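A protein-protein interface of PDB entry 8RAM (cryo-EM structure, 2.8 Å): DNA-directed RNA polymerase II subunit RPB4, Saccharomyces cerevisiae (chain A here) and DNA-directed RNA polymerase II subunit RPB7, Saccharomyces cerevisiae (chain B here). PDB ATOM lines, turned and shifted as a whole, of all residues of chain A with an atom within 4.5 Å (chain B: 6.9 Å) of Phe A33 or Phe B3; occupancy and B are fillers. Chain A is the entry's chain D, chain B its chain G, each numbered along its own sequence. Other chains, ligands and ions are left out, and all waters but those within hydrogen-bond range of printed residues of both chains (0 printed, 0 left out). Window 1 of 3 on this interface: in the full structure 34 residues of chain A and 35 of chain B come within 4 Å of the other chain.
The side-chain carboxylate (OE1) of Glu A32 lies within salt-bridge range of the side-chain amino group (NZ) of Lys B41. The side-chain amide nitrogen (NE2) of Gln A31 lies close to the side-chain amino group (NZ) of Lys B41.
O of Lys B80 sits at hydrogen-bond distance from N of Met B1 (3.0 Å). N of Ala B76 lies within hydrogen-bond range of O of Lys B5 (2.9 Å). OE1 of Gln A34 sits close to N of Glu A32 (3.2 Å). O of Phe B3 sits at hydrogen-bond distance from N of Val B78 (2.9 Å). N of Phe B2 lies within hydrogen-bond range of O of Val B78, 3.1 Å away. O of Gln A31 sits close to OE1 of Gln A34, at 2.8 Å.
Among the printed residues, merely in contact across the chains: Leu A50 with Phe B2 (2.9 Å), Phe A33 with Lys B5 (3.4 Å), Phe A175 with Met B1 (3.4 Å), Phe A175 with Phe B3 (3.5 Å), Glu A32 with Phe B42 (3.6 Å) and Phe A33 with Phe B3 (3.7 Å).
Gly A30 touches none of the printed residues of chain B. Of the printed residues of chain B, Gln A31 touches Lys B41. Printed residues of chain B within 4 Å of Glu A32: Lys B41 (2.6 Å) and Phe B42 (3.6 Å). Phe A33 touches two residues of chain B. Of chain A, only Phe A33 (3.7 Å) and Phe A175 (3.5 Å) come within 4 Å of Phe B3. Of the printed residues of chain A, Phe B42 touches Glu A32. The nearest residue of chain B that does not touch Phe A33 is Phe B82 (4.2 Å).
Of the 9 printed residues of chain A, 5 touch a printed residue of chain B. Printed residues of chain B that touch a printed residue of chain A: Met B1, Phe B2, Phe B3, Lys B5, Lys B41 and Phe B42. Hydrophobic or aromatic side chains of chain B that line the printed part of chain A: Met B1, Phe B2, Phe B3 and Phe B42. Among the printed residues, Asp or Glu carboxylates within 4 Å of a Lys or Arg side-chain nitrogen of the other chain: Glu A32 with Lys B41 (2.6 Å).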
ATOM      1  N   LEU A  29      26.648  22.970 -24.764  1.00  0.00           N
ATOM      2  CA  LEU A  29      25.688  22.304 -25.627  1.00  0.00           C
ATOM      3  C   LEU A  29      26.411  21.487 -26.699  1.00  0.00           C
ATOM      4  O   LEU A  29      27.629  21.562 -26.870  1.00  0.00           O
ATOM      5  CB  LEU A  29      24.756  23.326 -26.278  1.00  0.00           C
ATOM      6  CG  LEU A  29      23.678  23.967 -25.396  1.00  0.00           C
ATOM      7  CD1 LEU A  29      22.737  22.910 -24.832  1.00  0.00           C
ATOM      8  CD2 LEU A  29      24.294  24.791 -24.274  1.00  0.00           C
ATOM      9  N   GLY A  30      25.628  20.694 -27.429  1.00  0.00           N
ATOM     10  CA  GLY A  30      26.169  19.830 -28.455  1.00  0.00           C
ATOM     11  C   GLY A  30      26.492  20.575 -29.735  1.00  0.00           C
ATOM     12  O   GLY A  30      26.311  21.786 -29.861  1.00  0.00           O
ATOM     13  N   GLN A  31      26.986  19.813 -30.713  1.00  0.00           N
ATOM     14  CA  GLN A  31      27.374  20.399 -31.991  1.00  0.00           C
ATOM     15  C   GLN A  31      26.189  20.984 -32.746  1.00  0.00           C
ATOM     16  O   GLN A  31      26.389  21.815 -33.639  1.00  0.00           O
ATOM     17  CB  GLN A  31      28.085  19.350 -32.856  1.00  0.00           C
ATOM     18  CG  GLN A  31      27.311  18.050 -33.073  1.00  0.00           C
ATOM     19  CD  GLN A  31      26.162  18.196 -34.052  1.00  0.00           C
ATOM     20  OE1 GLN A  31      26.180  19.064 -34.925  1.00  0.00           O
ATOM     21  NE2 GLN A  31      25.153  17.346 -33.907  1.00  0.00           N
ATOM     22  N   GLU A  32      24.964  20.576 -32.413  1.00  0.00           N
ATOM     23  CA  GLU A  32      23.770  21.057 -33.095  1.00  0.00           C
ATOM     24  C   GLU A  32      22.954  22.045 -32.277  1.00  0.00           C
ATOM     25  O   GLU A  32      22.227  22.853 -32.859  1.00  0.00           O
ATOM     26  CB  GLU A  32      22.867  19.879 -33.483  1.00  0.00           C
ATOM     27  CG  GLU A  32      22.350  19.076 -32.300  1.00  0.00           C
ATOM     28  CD  GLU A  32      21.474  17.914 -32.722  1.00  0.00           C
ATOM     29  OE1 GLU A  32      21.354  17.670 -33.942  1.00  0.00           O
ATOM     30  OE2 GLU A  32      20.905  17.245 -31.835  1.00  0.00           O
ATOM     31  N   PHE A  33      23.054  22.004 -30.950  1.00  0.00           N
ATOM     32  CA  PHE A  33      22.295  22.909 -30.086  1.00  0.00           C
ATOM     33  C   PHE A  33      23.066  24.213 -29.869  1.00  0.00           C
ATOM     34  O   PHE A  33      23.402  24.602 -28.751  1.00  0.00           O
ATOM     35  CB  PHE A  33      21.976  22.227 -28.760  1.00  0.00           C
ATOM     36  CG  PHE A  33      21.065  21.041 -28.892  1.00  0.00           C
ATOM     37  CD1 PHE A  33      21.582  19.758 -28.959  1.00  0.00           C
ATOM     38  CD2 PHE A  33      19.692  21.208 -28.947  1.00  0.00           C
ATOM     39  CE1 PHE A  33      20.745  18.664 -29.080  1.00  0.00           C
ATOM     40  CE2 PHE A  33      18.851  20.119 -29.068  1.00  0.00           C
ATOM     41  CZ  PHE A  33      19.379  18.846 -29.135  1.00  0.00           C
ATOM     42  N   GLN A  34      23.344  24.892 -30.979  1.00  0.00           N
ATOM     43  CA  GLN A  34      24.030  26.172 -30.929  1.00  0.00           C
ATOM     44  C   GLN A  34      23.055  27.292 -30.581  1.00  0.00           C
ATOM     45  O   GLN A  34      21.834  27.147 -30.683  1.00  0.00           O
ATOM     46  CB  GLN A  34      24.712  26.473 -32.265  1.00  0.00           C
ATOM     47  CG  GLN A  34      26.146  25.977 -32.360  1.00  0.00           C
ATOM     48  CD  GLN A  34      26.264  24.477 -32.182  1.00  0.00           C
ATOM     49  OE1 GLN A  34      25.263  23.775 -32.040  1.00  0.00           O
ATOM     50  NE2 GLN A  34      27.494  23.977 -32.188  1.00  0.00           N
ATOM     51  N   LEU A  35      23.617  28.427 -30.163  1.00  0.00           N
ATOM     52  CA  LEU A  35      22.800  29.587 -29.826  1.00  0.00           C
ATOM     53  C   LEU A  35      22.093  30.167 -31.044  1.00  0.00           C
ATOM     54  O   LEU A  35      21.117  30.906 -30.884  1.00  0.00           O
ATOM     55  CB  LEU A  35      23.668  30.659 -29.163  1.00  0.00           C
ATOM     56  CG  LEU A  35      22.964  31.955 -28.752  1.00  0.00           C
ATOM     57  CD1 LEU A  35      23.490  32.440 -27.411  1.00  0.00           C
ATOM     58  CD2 LEU A  35      23.147  33.032 -29.811  1.00  0.00           C
ATOM     59  N   LEU A  50      10.213  27.415 -25.430  1.00  0.00           N
ATOM     60  CA  LEU A  50       8.834  27.581 -24.998  1.00  0.00           C
ATOM     61  C   LEU A  50       8.614  26.800 -23.710  1.00  0.00           C
ATOM     62  O   LEU A  50       9.316  25.826 -23.428  1.00  0.00           O
ATOM     63  CB  LEU A  50       7.841  27.115 -26.074  1.00  0.00           C
ATOM     64  CG  LEU A  50       7.660  25.608 -26.276  1.00  0.00           C
ATOM     65  CD1 LEU A  50       6.659  25.343 -27.390  1.00  0.00           C
ATOM     66  CD2 LEU A  50       8.982  24.925 -26.574  1.00  0.00           C
ATOM     67  N   PHE A 175      17.127  28.411 -22.862  1.00  0.00           N
ATOM     68  CA  PHE A 175      16.970  27.275 -21.961  1.00  0.00           C
ATOM     69  C   PHE A 175      16.790  27.737 -20.519  1.00  0.00           C
ATOM     70  O   PHE A 175      15.951  27.199 -19.786  1.00  0.00           O
ATOM     71  CB  PHE A 175      18.177  26.345 -22.083  1.00  0.00           C
ATOM     72  CG  PHE A 175      18.033  25.058 -21.325  1.00  0.00           C
ATOM     73  CD1 PHE A 175      18.764  24.831 -20.171  1.00  0.00           C
ATOM     74  CD2 PHE A 175      17.166  24.072 -21.767  1.00  0.00           C
ATOM     75  CE1 PHE A 175      18.635  23.646 -19.475  1.00  0.00           C
ATOM     76  CE2 PHE A 175      17.031  22.886 -21.072  1.00  0.00           C
ATOM     77  CZ  PHE A 175      17.767  22.673 -19.924  1.00  0.00           C
ATOM     78  N   MET B   1      15.109  19.696 -25.069  1.00  0.00           N
ATOM     79  CA  MET B   1      14.090  19.928 -24.007  1.00  0.00           C
ATOM     80  C   MET B   1      13.111  21.009 -24.452  1.00  0.00           C
ATOM     81  O   MET B   1      13.303  22.190 -24.164  1.00  0.00           O
ATOM     82  CB  MET B   1      14.768  20.324 -22.692  1.00  0.00           C
ATOM     83  CG  MET B   1      13.884  20.199 -21.454  1.00  0.00           C
ATOM     84  SD  MET B   1      12.598  21.461 -21.327  1.00  0.00           S
ATOM     85  CE  MET B   1      13.584  22.942 -21.127  1.00  0.00           C
ATOM     86  N   PHE B   2      12.058  20.596 -25.158  1.00  0.00           N
ATOM     87  CA  PHE B   2      11.039  21.512 -25.664  1.00  0.00           C
ATOM     88  C   PHE B   2      11.678  22.614 -26.513  1.00  0.00           C
ATOM     89  O   PHE B   2      11.638  23.800 -26.182  1.00  0.00           O
ATOM     90  CB  PHE B   2      10.223  22.107 -24.511  1.00  0.00           C
ATOM     91  CG  PHE B   2       9.520  21.079 -23.666  1.00  0.00           C
ATOM     92  CD1 PHE B   2       9.296  21.311 -22.319  1.00  0.00           C
ATOM     93  CD2 PHE B   2       9.080  19.886 -24.217  1.00  0.00           C
ATOM     94  CE1 PHE B   2       8.651  20.371 -21.537  1.00  0.00           C
ATOM     95  CE2 PHE B   2       8.434  18.943 -23.439  1.00  0.00           C
ATOM     96  CZ  PHE B   2       8.219  19.187 -22.098  1.00  0.00           C
ATOM     97  N   PHE B   3      12.282  22.192 -27.621  1.00  0.00           N
ATOM     98  CA  PHE B   3      12.931  23.095 -28.562  1.00  0.00           C
ATOM     99  C   PHE B   3      12.239  22.993 -29.912  1.00  0.00           C
ATOM    100  O   PHE B   3      11.960  21.888 -30.389  1.00  0.00           O
ATOM    101  CB  PHE B   3      14.421  22.766 -28.711  1.00  0.00           C
ATOM    102  CG  PHE B   3      15.211  22.914 -27.438  1.00  0.00           C
ATOM    103  CD1 PHE B   3      14.788  23.764 -26.428  1.00  0.00           C
ATOM    104  CD2 PHE B   3      16.386  22.204 -27.256  1.00  0.00           C
ATOM    105  CE1 PHE B   3      15.517  23.897 -25.263  1.00  0.00           C
ATOM    106  CE2 PHE B   3      17.120  22.334 -26.093  1.00  0.00           C
ATOM    107  CZ  PHE B   3      16.685  23.181 -25.096  1.00  0.00           C
ATOM    108  N   ILE B   4      11.962  24.143 -30.521  1.00  0.00           N
ATOM    109  CA  ILE B   4      11.349  24.214 -31.843  1.00  0.00           C
ATOM    110  C   ILE B   4      12.450  24.456 -32.864  1.00  0.00           C
ATOM    111  O   ILE B   4      13.265  25.374 -32.705  1.00  0.00           O
ATOM    112  CB  ILE B   4      10.278  25.318 -31.907  1.00  0.00           C
ATOM    113  CG1 ILE B   4       9.540  25.264 -33.248  1.00  0.00           C
ATOM    114  CG2 ILE B   4      10.904  26.695 -31.707  1.00  0.00           C
ATOM    115  CD1 ILE B   4       8.425  26.281 -33.374  1.00  0.00           C
ATOM    116  N   LYS B   5      12.482  23.633 -33.909  1.00  0.00           N
ATOM    117  CA  LYS B   5      13.532  23.730 -34.913  1.00  0.00           C
ATOM    118  C   LYS B   5      13.019  23.188 -36.239  1.00  0.00           C
ATOM    119  O   LYS B   5      12.007  22.486 -36.299  1.00  0.00           O
ATOM    120  CB  LYS B   5      14.793  22.974 -34.479  1.00  0.00           C
ATOM    121  CG  LYS B   5      14.547  21.522 -34.095  1.00  0.00           C
ATOM    122  CD  LYS B   5      15.845  20.783 -33.799  1.00  0.00           C
ATOM    123  CE  LYS B   5      16.551  21.344 -32.573  1.00  0.00           C
ATOM    124  NZ  LYS B   5      17.776  20.569 -32.234  1.00  0.00           N
ATOM    125  N   LEU B   7      13.284  20.775 -39.390  1.00  0.00           N
ATOM    126  CA  LEU B   7      13.775  19.453 -39.746  1.00  0.00           C
ATOM    127  C   LEU B   7      13.458  19.176 -41.208  1.00  0.00           C
ATOM    128  O   LEU B   7      12.365  19.496 -41.690  1.00  0.00           O
ATOM    129  CB  LEU B   7      13.148  18.364 -38.866  1.00  0.00           C
ATOM    130  CG  LEU B   7      13.469  18.401 -37.369  1.00  0.00           C
ATOM    131  CD1 LEU B   7      12.727  19.531 -36.670  1.00  0.00           C
ATOM    132  CD2 LEU B   7      13.139  17.062 -36.724  1.00  0.00           C
ATOM    133  N   GLY B  40      18.683   9.271 -31.374  1.00  0.00           N
ATOM    134  CA  GLY B  40      19.638   9.923 -30.496  1.00  0.00           C
ATOM    135  C   GLY B  40      20.167  11.228 -31.058  1.00  0.00           C
ATOM    136  O   GLY B  40      20.426  12.172 -30.308  1.00  0.00           O
ATOM    137  N   LYS B  41      20.336  11.301 -32.380  1.00  0.00           N
ATOM    138  CA  LYS B  41      20.859  12.515 -32.999  1.00  0.00           C
ATOM    139  C   LYS B  41      19.948  13.705 -32.720  1.00  0.00           C
ATOM    140  O   LYS B  41      20.363  14.693 -32.104  1.00  0.00           O
ATOM    141  CB  LYS B  41      21.024  12.296 -34.505  1.00  0.00           C
ATOM    142  CG  LYS B  41      21.584  13.491 -35.263  1.00  0.00           C
ATOM    143  CD  LYS B  41      22.976  13.866 -34.778  1.00  0.00           C
ATOM    144  CE  LYS B  41      23.583  14.966 -35.634  1.00  0.00           C
ATOM    145  NZ  LYS B  41      22.745  16.198 -35.642  1.00  0.00           N
ATOM    146  N   PHE B  42      18.697  13.625 -33.166  1.00  0.00           N
ATOM    147  CA  PHE B  42      17.728  14.696 -32.974  1.00  0.00           C
ATOM    148  C   PHE B  42      16.883  14.516 -31.720  1.00  0.00           C
ATOM    149  O   PHE B  42      15.976  15.321 -31.483  1.00  0.00           O
ATOM    150  CB  PHE B  42      16.807  14.797 -34.196  1.00  0.00           C
ATOM    151  CG  PHE B  42      17.529  15.077 -35.486  1.00  0.00           C
ATOM    152  CD1 PHE B  42      18.691  15.832 -35.502  1.00  0.00           C
ATOM    153  CD2 PHE B  42      17.042  14.584 -36.685  1.00  0.00           C
ATOM    154  CE1 PHE B  42      19.352  16.089 -36.688  1.00  0.00           C
ATOM    155  CE2 PHE B  42      17.699  14.837 -37.874  1.00  0.00           C
ATOM    156  CZ  PHE B  42      18.855  15.590 -37.875  1.00  0.00           C
ATOM    157  N   GLY B  43      17.153  13.490 -30.915  1.00  0.00           N
ATOM    158  CA  GLY B  43      16.345  13.265 -29.735  1.00  0.00           C
ATOM    159  C   GLY B  43      14.985  12.688 -30.092  1.00  0.00           C
ATOM    160  O   GLY B  43      14.805  12.024 -31.118  1.00  0.00           O
ATOM    161  N   ALA B  76       9.186  21.832 -36.205  1.00  0.00           N
ATOM    162  CA  ALA B  76       8.666  20.859 -35.258  1.00  0.00           C
ATOM    163  C   ALA B  76       9.259  21.114 -33.883  1.00  0.00           C
ATOM    164  O   ALA B  76      10.378  21.622 -33.752  1.00  0.00           O
ATOM    165  CB  ALA B  76       8.979  19.424 -35.702  1.00  0.00           C
ATOM    166  N   VAL B  77       8.496  20.749 -32.856  1.00  0.00           N
ATOM    167  CA  VAL B  77       8.927  20.848 -31.467  1.00  0.00           C
ATOM    168  C   VAL B  77       9.345  19.461 -31.003  1.00  0.00           C
ATOM    169  O   VAL B  77       8.618  18.479 -31.211  1.00  0.00           O
ATOM    170  CB  VAL B  77       7.814  21.422 -30.573  1.00  0.00           C
ATOM    171  CG1 VAL B  77       6.614  20.480 -30.522  1.00  0.00           C
ATOM    172  CG2 VAL B  77       8.344  21.694 -29.173  1.00  0.00           C
ATOM    173  N   VAL B  78      10.525  19.375 -30.385  1.00  0.00           N
ATOM    174  CA  VAL B  78      11.100  18.113 -29.949  1.00  0.00           C
ATOM    175  C   VAL B  78      11.557  18.251 -28.503  1.00  0.00           C
ATOM    176  O   VAL B  78      11.751  19.354 -27.987  1.00  0.00           O
ATOM    177  CB  VAL B  78      12.280  17.674 -30.845  1.00  0.00           C
ATOM    178  CG1 VAL B  78      11.868  17.691 -32.309  1.00  0.00           C
ATOM    179  CG2 VAL B  78      13.490  18.569 -30.614  1.00  0.00           C
ATOM    180  N   PHE B  79      11.727  17.103 -27.852  1.00  0.00           N
ATOM    181  CA  PHE B  79      12.161  17.028 -26.465  1.00  0.00           C
ATOM    182  C   PHE B  79      13.433  16.197 -26.374  1.00  0.00           C
ATOM    183  O   PHE B  79      13.547  15.146 -27.013  1.00  0.00           O
ATOM    184  CB  PHE B  79      11.071  16.419 -25.579  1.00  0.00           C
ATOM    185  CG  PHE B  79      11.477  16.255 -24.141  1.00  0.00           C
ATOM    186  CD1 PHE B  79      11.975  15.048 -23.681  1.00  0.00           C
ATOM    187  CD2 PHE B  79      11.359  17.309 -23.250  1.00  0.00           C
ATOM    188  CE1 PHE B  79      12.349  14.894 -22.360  1.00  0.00           C
ATOM    189  CE2 PHE B  79      11.731  17.161 -21.927  1.00  0.00           C
ATOM    190  CZ  PHE B  79      12.227  15.952 -21.483  1.00  0.00           C
ATOM    191  N   LYS B  80      14.388  16.673 -25.578  1.00  0.00           N
ATOM    192  CA  LYS B  80      15.663  15.989 -25.409  1.00  0.00           C
ATOM    193  C   LYS B  80      16.227  16.300 -24.027  1.00  0.00           C
ATOM    194  O   LYS B  80      16.639  17.439 -23.771  1.00  0.00           O
ATOM    195  CB  LYS B  80      16.646  16.416 -26.501  1.00  0.00           C
ATOM    196  CG  LYS B  80      17.713  15.378 -26.837  1.00  0.00           C
ATOM    197  CD  LYS B  80      18.645  15.111 -25.666  1.00  0.00           C
ATOM    198  CE  LYS B  80      19.787  14.191 -26.065  1.00  0.00           C
ATOM    199  NZ  LYS B  80      20.709  13.917 -24.928  1.00  0.00           N
ATOM    200  N   PHE B  82      18.783  16.553 -20.791  1.00  0.00           N
ATOM    201  CA  PHE B  82      20.200  16.844 -20.631  1.00  0.00           C
ATOM    202  C   PHE B  82      20.623  16.528 -19.204  1.00  0.00           C
ATOM    203  O   PHE B  82      19.813  16.572 -18.274  1.00  0.00           O
ATOM    204  CB  PHE B  82      20.516  18.310 -20.957  1.00  0.00           C
ATOM    205  CG  PHE B  82      20.254  18.682 -22.388  1.00  0.00           C
ATOM    206  CD1 PHE B  82      21.240  18.528 -23.350  1.00  0.00           C
ATOM    207  CD2 PHE B  82      19.024  19.188 -22.773  1.00  0.00           C
ATOM    208  CE1 PHE B  82      21.004  18.870 -24.667  1.00  0.00           C
ATOM    209  CE2 PHE B  82      18.782  19.532 -24.091  1.00  0.00           C
ATOM    210  CZ  PHE B  82      19.773  19.372 -25.037  1.00  0.00           C
